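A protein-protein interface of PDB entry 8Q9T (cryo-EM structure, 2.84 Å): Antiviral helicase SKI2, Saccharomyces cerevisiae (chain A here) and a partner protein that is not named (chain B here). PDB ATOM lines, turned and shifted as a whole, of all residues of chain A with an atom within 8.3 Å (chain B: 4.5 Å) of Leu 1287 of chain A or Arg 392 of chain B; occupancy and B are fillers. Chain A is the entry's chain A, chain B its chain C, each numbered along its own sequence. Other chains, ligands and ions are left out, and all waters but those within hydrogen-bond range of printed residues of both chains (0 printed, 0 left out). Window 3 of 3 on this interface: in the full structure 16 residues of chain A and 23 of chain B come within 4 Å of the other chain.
O of Val 4 of chain B is in hydrogen-bond range of N of Ala 394 of chain B, at 3.1 Å. The backbone carbonyl oxygen (O) of Leu 403 of chain A is in hydrogen-bond range of the backbone NH (N) of Ile 410 of chain A. NH1 of Arg 670 of chain A lies within hydrogen-bond range of O of Ala 1283 of chain A (3.2 Å). O of Ser 1284 of chain A sits at hydrogen-bond distance from NH1 of Arg 670 of chain A (3.2 Å). O of Ile 6 of chain B is in hydrogen-bond range of N of Arg 392 of chain B (2.7 Å).
OXT of Leu 1287 of chain A lies within salt-bridge range of NH1 of Arg 392 of chain B, at 3.3 Å.
Of the 10 printed residues of chain B, 4 touch a printed residue of chain A. Printed residues of chain B that touch a printed residue of chain A: Val 4, Ile 6, Arg 392 and Gly 395. Hydrophobic or aromatic side chains of chain B within 4 Å of the printed part of chain A: Val 4 and Ile 6. Hydrophobic or aromatic side chains of chain A that line the printed part of chain B: Ile 410 and Ala 1283. Among the printed residues, 5 pairs touch across the chains.
Of the printed residues of chain B, Ile 410 of chain A touches Gly 395 (3.7 Å). Of the printed residues of chain B, Arg 670 of chain A touches Ile 6 (3.98 Å). Printed residues of chain B within 4 Å of Leu 1287 of chain A: Arg 392. Of the printed residues of chain A, Ile 6 of chain B touches Arg 670 and Ala 1283. Arg 392 of chain B touches one residue of chain A. The nearest printed residue of chain B that does not touch Leu 1287 of chain A is Ala 394 of chain B (4.01 Å).
Gly 395 of chain B touches Ile 410 of chain A (CA to CG2, 3.7 Å). Arg 670 of chain A touches Ile 6 of chain B (CZ to CG2, 3.98 Å). CG1 of Val 4 of chain B touches CB of Ala 1283 of chain A (3.7 Å). Ala 1283 of chain A touches Ile 6 of chain B (CB to CG1, 3.9 Å).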
ATOM      1  N   SER A 385     -17.685  11.053 -19.690  1.00  0.00           N
ATOM      2  CA  SER A 385     -17.003  12.160 -20.349  1.00  0.00           C
ATOM      3  C   SER A 385     -16.653  13.264 -19.360  1.00  0.00           C
ATOM      4  O   SER A 385     -15.540  13.800 -19.389  1.00  0.00           O
ATOM      5  CB  SER A 385     -17.874  12.704 -21.481  1.00  0.00           C
ATOM      6  OG  SER A 385     -18.083  11.717 -22.475  1.00  0.00           O
ATOM      7  N   ASN A 386     -17.584  13.610 -18.469  1.00  0.00           N
ATOM      8  CA  ASN A 386     -17.323  14.663 -17.491  1.00  0.00           C
ATOM      9  C   ASN A 386     -16.255  14.243 -16.487  1.00  0.00           C
ATOM     10  O   ASN A 386     -15.371  15.038 -16.137  1.00  0.00           O
ATOM     11  CB  ASN A 386     -18.619  15.030 -16.775  1.00  0.00           C
ATOM     12  CG  ASN A 386     -19.723  15.418 -17.735  1.00  0.00           C
ATOM     13  OD1 ASN A 386     -19.493  16.142 -18.702  1.00  0.00           O
ATOM     14  ND2 ASN A 386     -20.929  14.927 -17.480  1.00  0.00           N
ATOM     15  N   GLN A 387     -16.325  13.000 -16.008  1.00  0.00           N
ATOM     16  CA  GLN A 387     -15.311  12.507 -15.083  1.00  0.00           C
ATOM     17  C   GLN A 387     -13.936  12.506 -15.730  1.00  0.00           C
ATOM     18  O   GLN A 387     -12.948  12.917 -15.108  1.00  0.00           O
ATOM     19  CB  GLN A 387     -15.673  11.103 -14.609  1.00  0.00           C
ATOM     20  CG  GLN A 387     -16.746  11.059 -13.549  1.00  0.00           C
ATOM     21  CD  GLN A 387     -16.829   9.710 -12.869  1.00  0.00           C
ATOM     22  OE1 GLN A 387     -17.637   8.861 -13.244  1.00  0.00           O
ATOM     23  NE2 GLN A 387     -15.988   9.504 -11.863  1.00  0.00           N
ATOM     24  N   PHE A 389     -12.959  14.389 -18.246  1.00  0.00           N
ATOM     25  CA  PHE A 389     -12.566  15.782 -18.426  1.00  0.00           C
ATOM     26  C   PHE A 389     -11.937  16.340 -17.157  1.00  0.00           C
ATOM     27  O   PHE A 389     -10.843  16.918 -17.190  1.00  0.00           O
ATOM     28  CB  PHE A 389     -13.789  16.601 -18.841  1.00  0.00           C
ATOM     29  CG  PHE A 389     -13.540  18.076 -18.932  1.00  0.00           C
ATOM     30  CD1 PHE A 389     -12.965  18.627 -20.063  1.00  0.00           C
ATOM     31  CD2 PHE A 389     -13.909  18.918 -17.898  1.00  0.00           C
ATOM     32  CE1 PHE A 389     -12.746  19.984 -20.152  1.00  0.00           C
ATOM     33  CE2 PHE A 389     -13.690  20.274 -17.983  1.00  0.00           C
ATOM     34  CZ  PHE A 389     -13.110  20.808 -19.114  1.00  0.00           C
ATOM     35  N   ARG A 390     -12.611  16.161 -16.019  1.00  0.00           N
ATOM     36  CA  ARG A 390     -12.073  16.668 -14.760  1.00  0.00           C
ATOM     37  C   ARG A 390     -10.750  15.991 -14.408  1.00  0.00           C
ATOM     38  O   ARG A 390      -9.793  16.661 -13.999  1.00  0.00           O
ATOM     39  CB  ARG A 390     -13.097  16.480 -13.641  1.00  0.00           C
ATOM     40  CG  ARG A 390     -12.623  16.903 -12.257  1.00  0.00           C
ATOM     41  CD  ARG A 390     -12.075  18.323 -12.230  1.00  0.00           C
ATOM     42  NE  ARG A 390     -12.934  19.278 -12.918  1.00  0.00           N
ATOM     43  CZ  ARG A 390     -12.528  20.458 -13.367  1.00  0.00           C
ATOM     44  NH1 ARG A 390     -11.279  20.866 -13.210  1.00  0.00           N
ATOM     45  NH2 ARG A 390     -13.397  21.250 -13.989  1.00  0.00           N
ATOM     46  N   LYS A 393      -7.943  17.251 -16.750  1.00  0.00           N
ATOM     47  CA  LYS A 393      -7.590  18.632 -16.452  1.00  0.00           C
ATOM     48  C   LYS A 393      -6.824  18.742 -15.140  1.00  0.00           C
ATOM     49  O   LYS A 393      -5.978  19.630 -14.992  1.00  0.00           O
ATOM     50  CB  LYS A 393      -8.847  19.500 -16.421  1.00  0.00           C
ATOM     51  CG  LYS A 393      -8.569  20.985 -16.513  1.00  0.00           C
ATOM     52  CD  LYS A 393      -9.817  21.761 -16.873  1.00  0.00           C
ATOM     53  CE  LYS A 393      -9.913  21.979 -18.370  1.00  0.00           C
ATOM     54  NZ  LYS A 393      -8.941  22.997 -18.855  1.00  0.00           N
ATOM     55  N   GLY A 402     -10.291  19.557 -23.715  1.00  0.00           N
ATOM     56  CA  GLY A 402     -11.581  20.043 -24.140  1.00  0.00           C
ATOM     57  C   GLY A 402     -12.632  18.955 -24.057  1.00  0.00           C
ATOM     58  O   GLY A 402     -12.329  17.774 -23.901  1.00  0.00           O
ATOM     59  N   LEU A 403     -13.889  19.380 -24.163  1.00  0.00           N
ATOM     60  CA  LEU A 403     -15.026  18.476 -24.063  1.00  0.00           C
ATOM     61  C   LEU A 403     -16.053  18.849 -25.117  1.00  0.00           C
ATOM     62  O   LEU A 403     -16.450  20.013 -25.212  1.00  0.00           O
ATOM     63  CB  LEU A 403     -15.649  18.533 -22.663  1.00  0.00           C
ATOM     64  CG  LEU A 403     -16.930  17.744 -22.391  1.00  0.00           C
ATOM     65  CD1 LEU A 403     -16.651  16.258 -22.331  1.00  0.00           C
ATOM     66  CD2 LEU A 403     -17.558  18.216 -21.099  1.00  0.00           C
ATOM     67  N   THR A 405     -19.824  17.715 -26.596  1.00  0.00           N
ATOM     68  CA  THR A 405     -21.043  16.927 -26.479  1.00  0.00           C
ATOM     69  C   THR A 405     -22.090  17.447 -27.456  1.00  0.00           C
ATOM     70  O   THR A 405     -21.777  18.267 -28.325  1.00  0.00           O
ATOM     71  CB  THR A 405     -21.574  16.947 -25.044  1.00  0.00           C
ATOM     72  OG1 THR A 405     -22.830  16.259 -24.991  1.00  0.00           O
ATOM     73  CG2 THR A 405     -21.764  18.364 -24.563  1.00  0.00           C
ATOM     74  N   VAL A 408     -23.006  21.353 -25.713  1.00  0.00           N
ATOM     75  CA  VAL A 408     -21.959  22.165 -25.104  1.00  0.00           C
ATOM     76  C   VAL A 408     -20.629  21.913 -25.799  1.00  0.00           C
ATOM     77  O   VAL A 408     -20.345  20.815 -26.284  1.00  0.00           O
ATOM     78  CB  VAL A 408     -21.859  21.884 -23.590  1.00  0.00           C
ATOM     79  N   GLN A 409     -19.806  22.958 -25.848  1.00  0.00           N
ATOM     80  CA  GLN A 409     -18.439  22.878 -26.348  1.00  0.00           C
ATOM     81  C   GLN A 409     -17.546  23.620 -25.369  1.00  0.00           C
ATOM     82  O   GLN A 409     -17.797  24.790 -25.069  1.00  0.00           O
ATOM     83  CB  GLN A 409     -18.316  23.486 -27.747  1.00  0.00           C
ATOM     84  CG  GLN A 409     -18.822  22.604 -28.868  1.00  0.00           C
ATOM     85  CD  GLN A 409     -18.649  23.247 -30.228  1.00  0.00           C
ATOM     86  OE1 GLN A 409     -18.063  24.322 -30.348  1.00  0.00           O
ATOM     87  NE2 GLN A 409     -19.163  22.594 -31.261  1.00  0.00           N
ATOM     88  N   ILE A 410     -16.515  22.949 -24.868  1.00  0.00           N
ATOM     89  CA  ILE A 410     -15.594  23.528 -23.899  1.00  0.00           C
ATOM     90  C   ILE A 410     -14.186  23.397 -24.457  1.00  0.00           C
ATOM     91  O   ILE A 410     -13.724  22.282 -24.726  1.00  0.00           O
ATOM     92  CB  ILE A 410     -15.709  22.846 -22.527  1.00  0.00           C
ATOM     93  CG1 ILE A 410     -17.125  23.009 -21.974  1.00  0.00           C
ATOM     94  CG2 ILE A 410     -14.684  23.412 -21.563  1.00  0.00           C
ATOM     95  CD1 ILE A 410     -17.242  22.733 -20.507  1.00  0.00           C
ATOM     96  N   ARG A 670     -26.491  26.772  -7.708  1.00  0.00           N
ATOM     97  CA  ARG A 670     -26.883  27.043  -9.084  1.00  0.00           C
ATOM     98  C   ARG A 670     -28.371  26.839  -9.340  1.00  0.00           C
ATOM     99  O   ARG A 670     -28.846  27.200 -10.421  1.00  0.00           O
ATOM    100  CB  ARG A 670     -26.075  26.156 -10.032  1.00  0.00           C
ATOM    101  CG  ARG A 670     -26.118  24.678  -9.675  1.00  0.00           C
ATOM    102  CD  ARG A 670     -25.064  23.889 -10.428  1.00  0.00           C
ATOM    103  NE  ARG A 670     -23.762  23.961  -9.777  1.00  0.00           N
ATOM    104  CZ  ARG A 670     -22.613  23.667 -10.368  1.00  0.00           C
ATOM    105  NH1 ARG A 670     -22.566  23.272 -11.627  1.00  0.00           N
ATOM    106  NH2 ARG A 670     -21.483  23.773  -9.676  1.00  0.00           N
ATOM    107  N   GLU A 705     -23.951  13.127  -9.412  1.00  0.00           N
ATOM    108  CA  GLU A 705     -22.631  13.752  -9.404  1.00  0.00           C
ATOM    109  C   GLU A 705     -22.206  14.128  -7.991  1.00  0.00           C
ATOM    110  O   GLU A 705     -21.050  13.920  -7.606  1.00  0.00           O
ATOM    111  CB  GLU A 705     -22.625  14.983 -10.306  1.00  0.00           C
ATOM    112  CG  GLU A 705     -22.754  14.672 -11.777  1.00  0.00           C
ATOM    113  CD  GLU A 705     -23.063  15.901 -12.600  1.00  0.00           C
ATOM    114  OE1 GLU A 705     -23.348  16.958 -12.003  1.00  0.00           O
ATOM    115  OE2 GLU A 705     -23.025  15.811 -13.844  1.00  0.00           O
ATOM    116  N   ILE A 709     -18.910  12.527  -6.171  1.00  0.00           N
ATOM    117  CA  ILE A 709     -17.824  13.387  -5.712  1.00  0.00           C
ATOM    118  C   ILE A 709     -17.600  13.222  -4.213  1.00  0.00           C
ATOM    119  O   ILE A 709     -16.456  13.153  -3.750  1.00  0.00           O
ATOM    120  CB  ILE A 709     -18.105  14.851  -6.089  1.00  0.00           C
ATOM    121  CG1 ILE A 709     -18.056  15.022  -7.607  1.00  0.00           C
ATOM    122  CG2 ILE A 709     -17.103  15.773  -5.425  1.00  0.00           C
ATOM    123  CD1 ILE A 709     -18.079  16.456  -8.063  1.00  0.00           C
ATOM    124  N   ALA A1282     -29.241  21.682 -15.915  1.00  0.00           N
ATOM    125  CA  ALA A1282     -28.274  22.316 -15.032  1.00  0.00           C
ATOM    126  C   ALA A1282     -26.859  21.861 -15.365  1.00  0.00           C
ATOM    127  O   ALA A1282     -26.624  20.712 -15.747  1.00  0.00           O
ATOM    128  CB  ALA A1282     -28.593  21.999 -13.573  1.00  0.00           C
ATOM    129  N   ALA A1283     -25.911  22.781 -15.210  1.00  0.00           N
ATOM    130  CA  ALA A1283     -24.522  22.500 -15.539  1.00  0.00           C
ATOM    131  C   ALA A1283     -23.951  21.428 -14.619  1.00  0.00           C
ATOM    132  O   ALA A1283     -24.354  21.288 -13.463  1.00  0.00           O
ATOM    133  CB  ALA A1283     -23.682  23.771 -15.441  1.00  0.00           C
ATOM    134  N   SER A1284     -23.006  20.662 -15.152  1.00  0.00           N
ATOM    135  CA  SER A1284     -22.424  19.557 -14.406  1.00  0.00           C
ATOM    136  C   SER A1284     -21.524  20.067 -13.288  1.00  0.00           C
ATOM    137  O   SER A1284     -20.922  21.139 -13.381  1.00  0.00           O
ATOM    138  CB  SER A1284     -21.629  18.647 -15.340  1.00  0.00           C
ATOM    139  OG  SER A1284     -21.161  17.501 -14.657  1.00  0.00           O
ATOM    140  N   LEU A1285     -21.438  19.281 -12.217  1.00  0.00           N
ATOM    141  CA  LEU A1285     -20.571  19.601 -11.092  1.00  0.00           C
ATOM    142  C   LEU A1285     -19.099  19.358 -11.393  1.00  0.00           C
ATOM    143  O   LEU A1285     -18.248  19.746 -10.587  1.00  0.00           O
ATOM    144  CB  LEU A1285     -20.988  18.792  -9.863  1.00  0.00           C
ATOM    145  CG  LEU A1285     -21.888  19.477  -8.833  1.00  0.00           C
ATOM    146  CD1 LEU A1285     -23.152  19.993  -9.476  1.00  0.00           C
ATOM    147  CD2 LEU A1285     -22.225  18.511  -7.716  1.00  0.00           C
ATOM    148  N   TYR A1286     -18.779  18.724 -12.520  1.00  0.00           N
ATOM    149  CA  TYR A1286     -17.400  18.543 -12.951  1.00  0.00           C
ATOM    150  C   TYR A1286     -16.878  19.708 -13.782  1.00  0.00           C
ATOM    151  O   TYR A1286     -15.665  19.802 -13.991  1.00  0.00           O
ATOM    152  CB  TYR A1286     -17.261  17.249 -13.756  1.00  0.00           C
ATOM    153  CG  TYR A1286     -17.509  15.993 -12.957  1.00  0.00           C
ATOM    154  CD1 TYR A1286     -16.556  15.513 -12.071  1.00  0.00           C
ATOM    155  CD2 TYR A1286     -18.691  15.287 -13.090  1.00  0.00           C
ATOM    156  CE1 TYR A1286     -16.778  14.366 -11.340  1.00  0.00           C
ATOM    157  CE2 TYR A1286     -18.921  14.142 -12.364  1.00  0.00           C
ATOM    158  CZ  TYR A1286     -17.962  13.685 -11.490  1.00  0.00           C
ATOM    159  OH  TYR A1286     -18.191  12.541 -10.765  1.00  0.00           O
ATOM    160  N   LEU A1287     -17.750  20.588 -14.261  1.00  0.00           N
ATOM    161  CA  LEU A1287     -17.317  21.758 -15.014  1.00  0.00           C
ATOM    162  C   LEU A1287     -17.147  22.961 -14.093  1.00  0.00           C
ATOM    163  O   LEU A1287     -17.486  22.910 -12.911  1.00  0.00           O
ATOM    164  CB  LEU A1287     -18.313  22.092 -16.126  1.00  0.00           C
ATOM    165  CG  LEU A1287     -18.820  20.934 -16.980  1.00  0.00           C
ATOM    166  CD1 LEU A1287     -19.933  21.403 -17.895  1.00  0.00           C
ATOM    167  CD2 LEU A1287     -17.686  20.326 -17.780  1.00  0.00           C
ATOM    168  OXT LEU A1287     -16.666  24.014 -14.514  1.00  0.00           O
ATOM    169  N   VAL B   4     -21.543  27.804 -21.262  1.00  0.00           N
ATOM    170  CA  VAL B   4     -22.041  27.383 -19.959  1.00  0.00           C
ATOM    171  C   VAL B   4     -21.684  28.455 -18.939  1.00  0.00           C
ATOM    172  O   VAL B   4     -20.518  28.846 -18.827  1.00  0.00           O
ATOM    173  CB  VAL B   4     -21.461  26.020 -19.535  1.00  0.00           C
ATOM    174  CG1 VAL B   4     -22.017  25.603 -18.188  1.00  0.00           C
ATOM    175  CG2 VAL B   4     -21.757  24.963 -20.585  1.00  0.00           C
ATOM    176  N   PHE B   5     -22.686  28.926 -18.199  1.00  0.00           N
ATOM    177  CA  PHE B   5     -22.496  29.930 -17.160  1.00  0.00           C
ATOM    178  C   PHE B   5     -23.087  29.410 -15.861  1.00  0.00           C
ATOM    179  O   PHE B   5     -24.229  28.942 -15.840  1.00  0.00           O
ATOM    180  CB  PHE B   5     -23.142  31.263 -17.549  1.00  0.00           C
ATOM    181  CG  PHE B   5     -22.452  31.960 -18.684  1.00  0.00           C
ATOM    182  CD1 PHE B   5     -21.396  32.820 -18.446  1.00  0.00           C
ATOM    183  CD2 PHE B   5     -22.854  31.749 -19.990  1.00  0.00           C
ATOM    184  CE1 PHE B   5     -20.756  33.457 -19.487  1.00  0.00           C
ATOM    185  CE2 PHE B   5     -22.215  32.383 -21.034  1.00  0.00           C
ATOM    186  CZ  PHE B   5     -21.167  33.238 -20.783  1.00  0.00           C
ATOM    187  N   ILE B   6     -22.314  29.497 -14.781  1.00  0.00           N
ATOM    188  CA  ILE B   6     -22.698  28.972 -13.477  1.00  0.00           C
ATOM    189  C   ILE B   6     -22.782  30.131 -12.495  1.00  0.00           C
ATOM    190  O   ILE B   6     -21.874  30.968 -12.439  1.00  0.00           O
ATOM    191  CB  ILE B   6     -21.705  27.907 -12.975  1.00  0.00           C
ATOM    192  CG1 ILE B   6     -21.633  26.729 -13.945  1.00  0.00           C
ATOM    193  CG2 ILE B   6     -22.092  27.418 -11.593  1.00  0.00           C
ATOM    194  CD1 ILE B   6     -20.376  26.699 -14.775  1.00  0.00           C
ATOM    195  N   THR B   8     -22.373  32.072  -9.129  1.00  0.00           N
ATOM    196  CA  THR B   8     -21.303  32.022  -8.140  1.00  0.00           C
ATOM    197  C   THR B   8     -21.711  32.646  -6.812  1.00  0.00           C
ATOM    198  O   THR B   8     -21.670  31.978  -5.777  1.00  0.00           O
ATOM    199  CB  THR B   8     -20.055  32.722  -8.692  1.00  0.00           C
ATOM    200  OG1 THR B   8     -19.475  31.923  -9.727  1.00  0.00           O
ATOM    201  CG2 THR B   8     -19.033  32.930  -7.594  1.00  0.00           C
ATOM    202  N   GLU B 377     -13.411  33.910 -17.440  1.00  0.00           N
ATOM    203  CA  GLU B 377     -14.123  35.173 -17.352  1.00  0.00           C
ATOM    204  C   GLU B 377     -15.285  35.071 -16.366  1.00  0.00           C
ATOM    205  O   GLU B 377     -15.610  34.002 -15.845  1.00  0.00           O
ATOM    206  CB  GLU B 377     -14.635  35.595 -18.725  1.00  0.00           C
ATOM    207  CG  GLU B 377     -13.564  36.130 -19.649  1.00  0.00           C
ATOM    208  CD  GLU B 377     -13.836  35.797 -21.100  1.00  0.00           C
ATOM    209  OE1 GLU B 377     -14.772  35.016 -21.364  1.00  0.00           O
ATOM    210  OE2 GLU B 377     -13.113  36.314 -21.977  1.00  0.00           O
ATOM    211  N   PHE B 391     -21.775  35.488 -12.077  1.00  0.00           N
ATOM    212  CA  PHE B 391     -21.746  34.238 -12.822  1.00  0.00           C
ATOM    213  C   PHE B 391     -20.316  33.898 -13.218  1.00  0.00           C
ATOM    214  O   PHE B 391     -19.434  34.757 -13.245  1.00  0.00           O
ATOM    215  CB  PHE B 391     -22.632  34.306 -14.073  1.00  0.00           C
ATOM    216  CG  PHE B 391     -24.098  34.411 -13.772  1.00  0.00           C
ATOM    217  CD1 PHE B 391     -24.873  33.275 -13.640  1.00  0.00           C
ATOM    218  CD2 PHE B 391     -24.702  35.646 -13.623  1.00  0.00           C
ATOM    219  CE1 PHE B 391     -26.216  33.370 -13.362  1.00  0.00           C
ATOM    220  CE2 PHE B 391     -26.047  35.744 -13.345  1.00  0.00           C
ATOM    221  CZ  PHE B 391     -26.803  34.606 -13.214  1.00  0.00           C
ATOM    222  N   ARG B 392     -20.099  32.622 -13.527  1.00  0.00           N
ATOM    223  CA  ARG B 392     -18.790  32.095 -13.886  1.00  0.00           C
ATOM    224  C   ARG B 392     -18.905  31.279 -15.164  1.00  0.00           C
ATOM    225  O   ARG B 392     -19.906  30.593 -15.379  1.00  0.00           O
ATOM    226  CB  ARG B 392     -18.225  31.229 -12.754  1.00  0.00           C
ATOM    227  CG  ARG B 392     -17.070  30.340 -13.156  1.00  0.00           C
ATOM    228  CD  ARG B 392     -16.524  29.572 -11.974  1.00  0.00           C
ATOM    229  NE  ARG B 392     -17.387  28.464 -11.585  1.00  0.00           N
ATOM    230  CZ  ARG B 392     -17.241  27.216 -12.009  1.00  0.00           C
ATOM    231  NH1 ARG B 392     -16.295  26.887 -12.870  1.00  0.00           N
ATOM    232  NH2 ARG B 392     -18.064  26.277 -11.555  1.00  0.00           N
ATOM    233  N   GLU B 393     -17.878  31.346 -16.008  1.00  0.00           N
ATOM    234  CA  GLU B 393     -17.866  30.604 -17.262  1.00  0.00           C
ATOM    235  C   GLU B 393     -17.156  29.268 -17.078  1.00  0.00           C
ATOM    236  O   GLU B 393     -16.038  29.216 -16.556  1.00  0.00           O
ATOM    237  CB  GLU B 393     -17.186  31.415 -18.362  1.00  0.00           C
ATOM    238  CG  GLU B 393     -17.611  31.020 -19.760  1.00  0.00           C
ATOM    239  CD  GLU B 393     -16.705  31.596 -20.828  1.00  0.00           C
ATOM    240  OE1 GLU B 393     -15.591  31.063 -21.012  1.00  0.00           O
ATOM    241  OE2 GLU B 393     -17.106  32.579 -21.484  1.00  0.00           O
ATOM    242  N   ALA B 394     -17.809  28.194 -17.511  1.00  0.00           N
ATOM    243  CA  ALA B 394     -17.232  26.864 -17.405  1.00  0.00           C
ATOM    244  C   ALA B 394     -16.044  26.708 -18.348  1.00  0.00           C
ATOM    245  O   ALA B 394     -16.003  27.286 -19.436  1.00  0.00           O
ATOM    246  CB  ALA B 394     -18.283  25.802 -17.718  1.00  0.00           C
ATOM    247  N   GLY B 395     -15.071  25.911 -17.917  1.00  0.00           N
ATOM    248  CA  GLY B 395     -13.883  25.665 -18.712  1.00  0.00           C
ATOM    249  C   GLY B 395     -12.594  25.893 -17.951  1.00  0.00           C
ATOM    250  O   GLY B 395     -12.610  26.117 -16.741  1.00  0.00           O
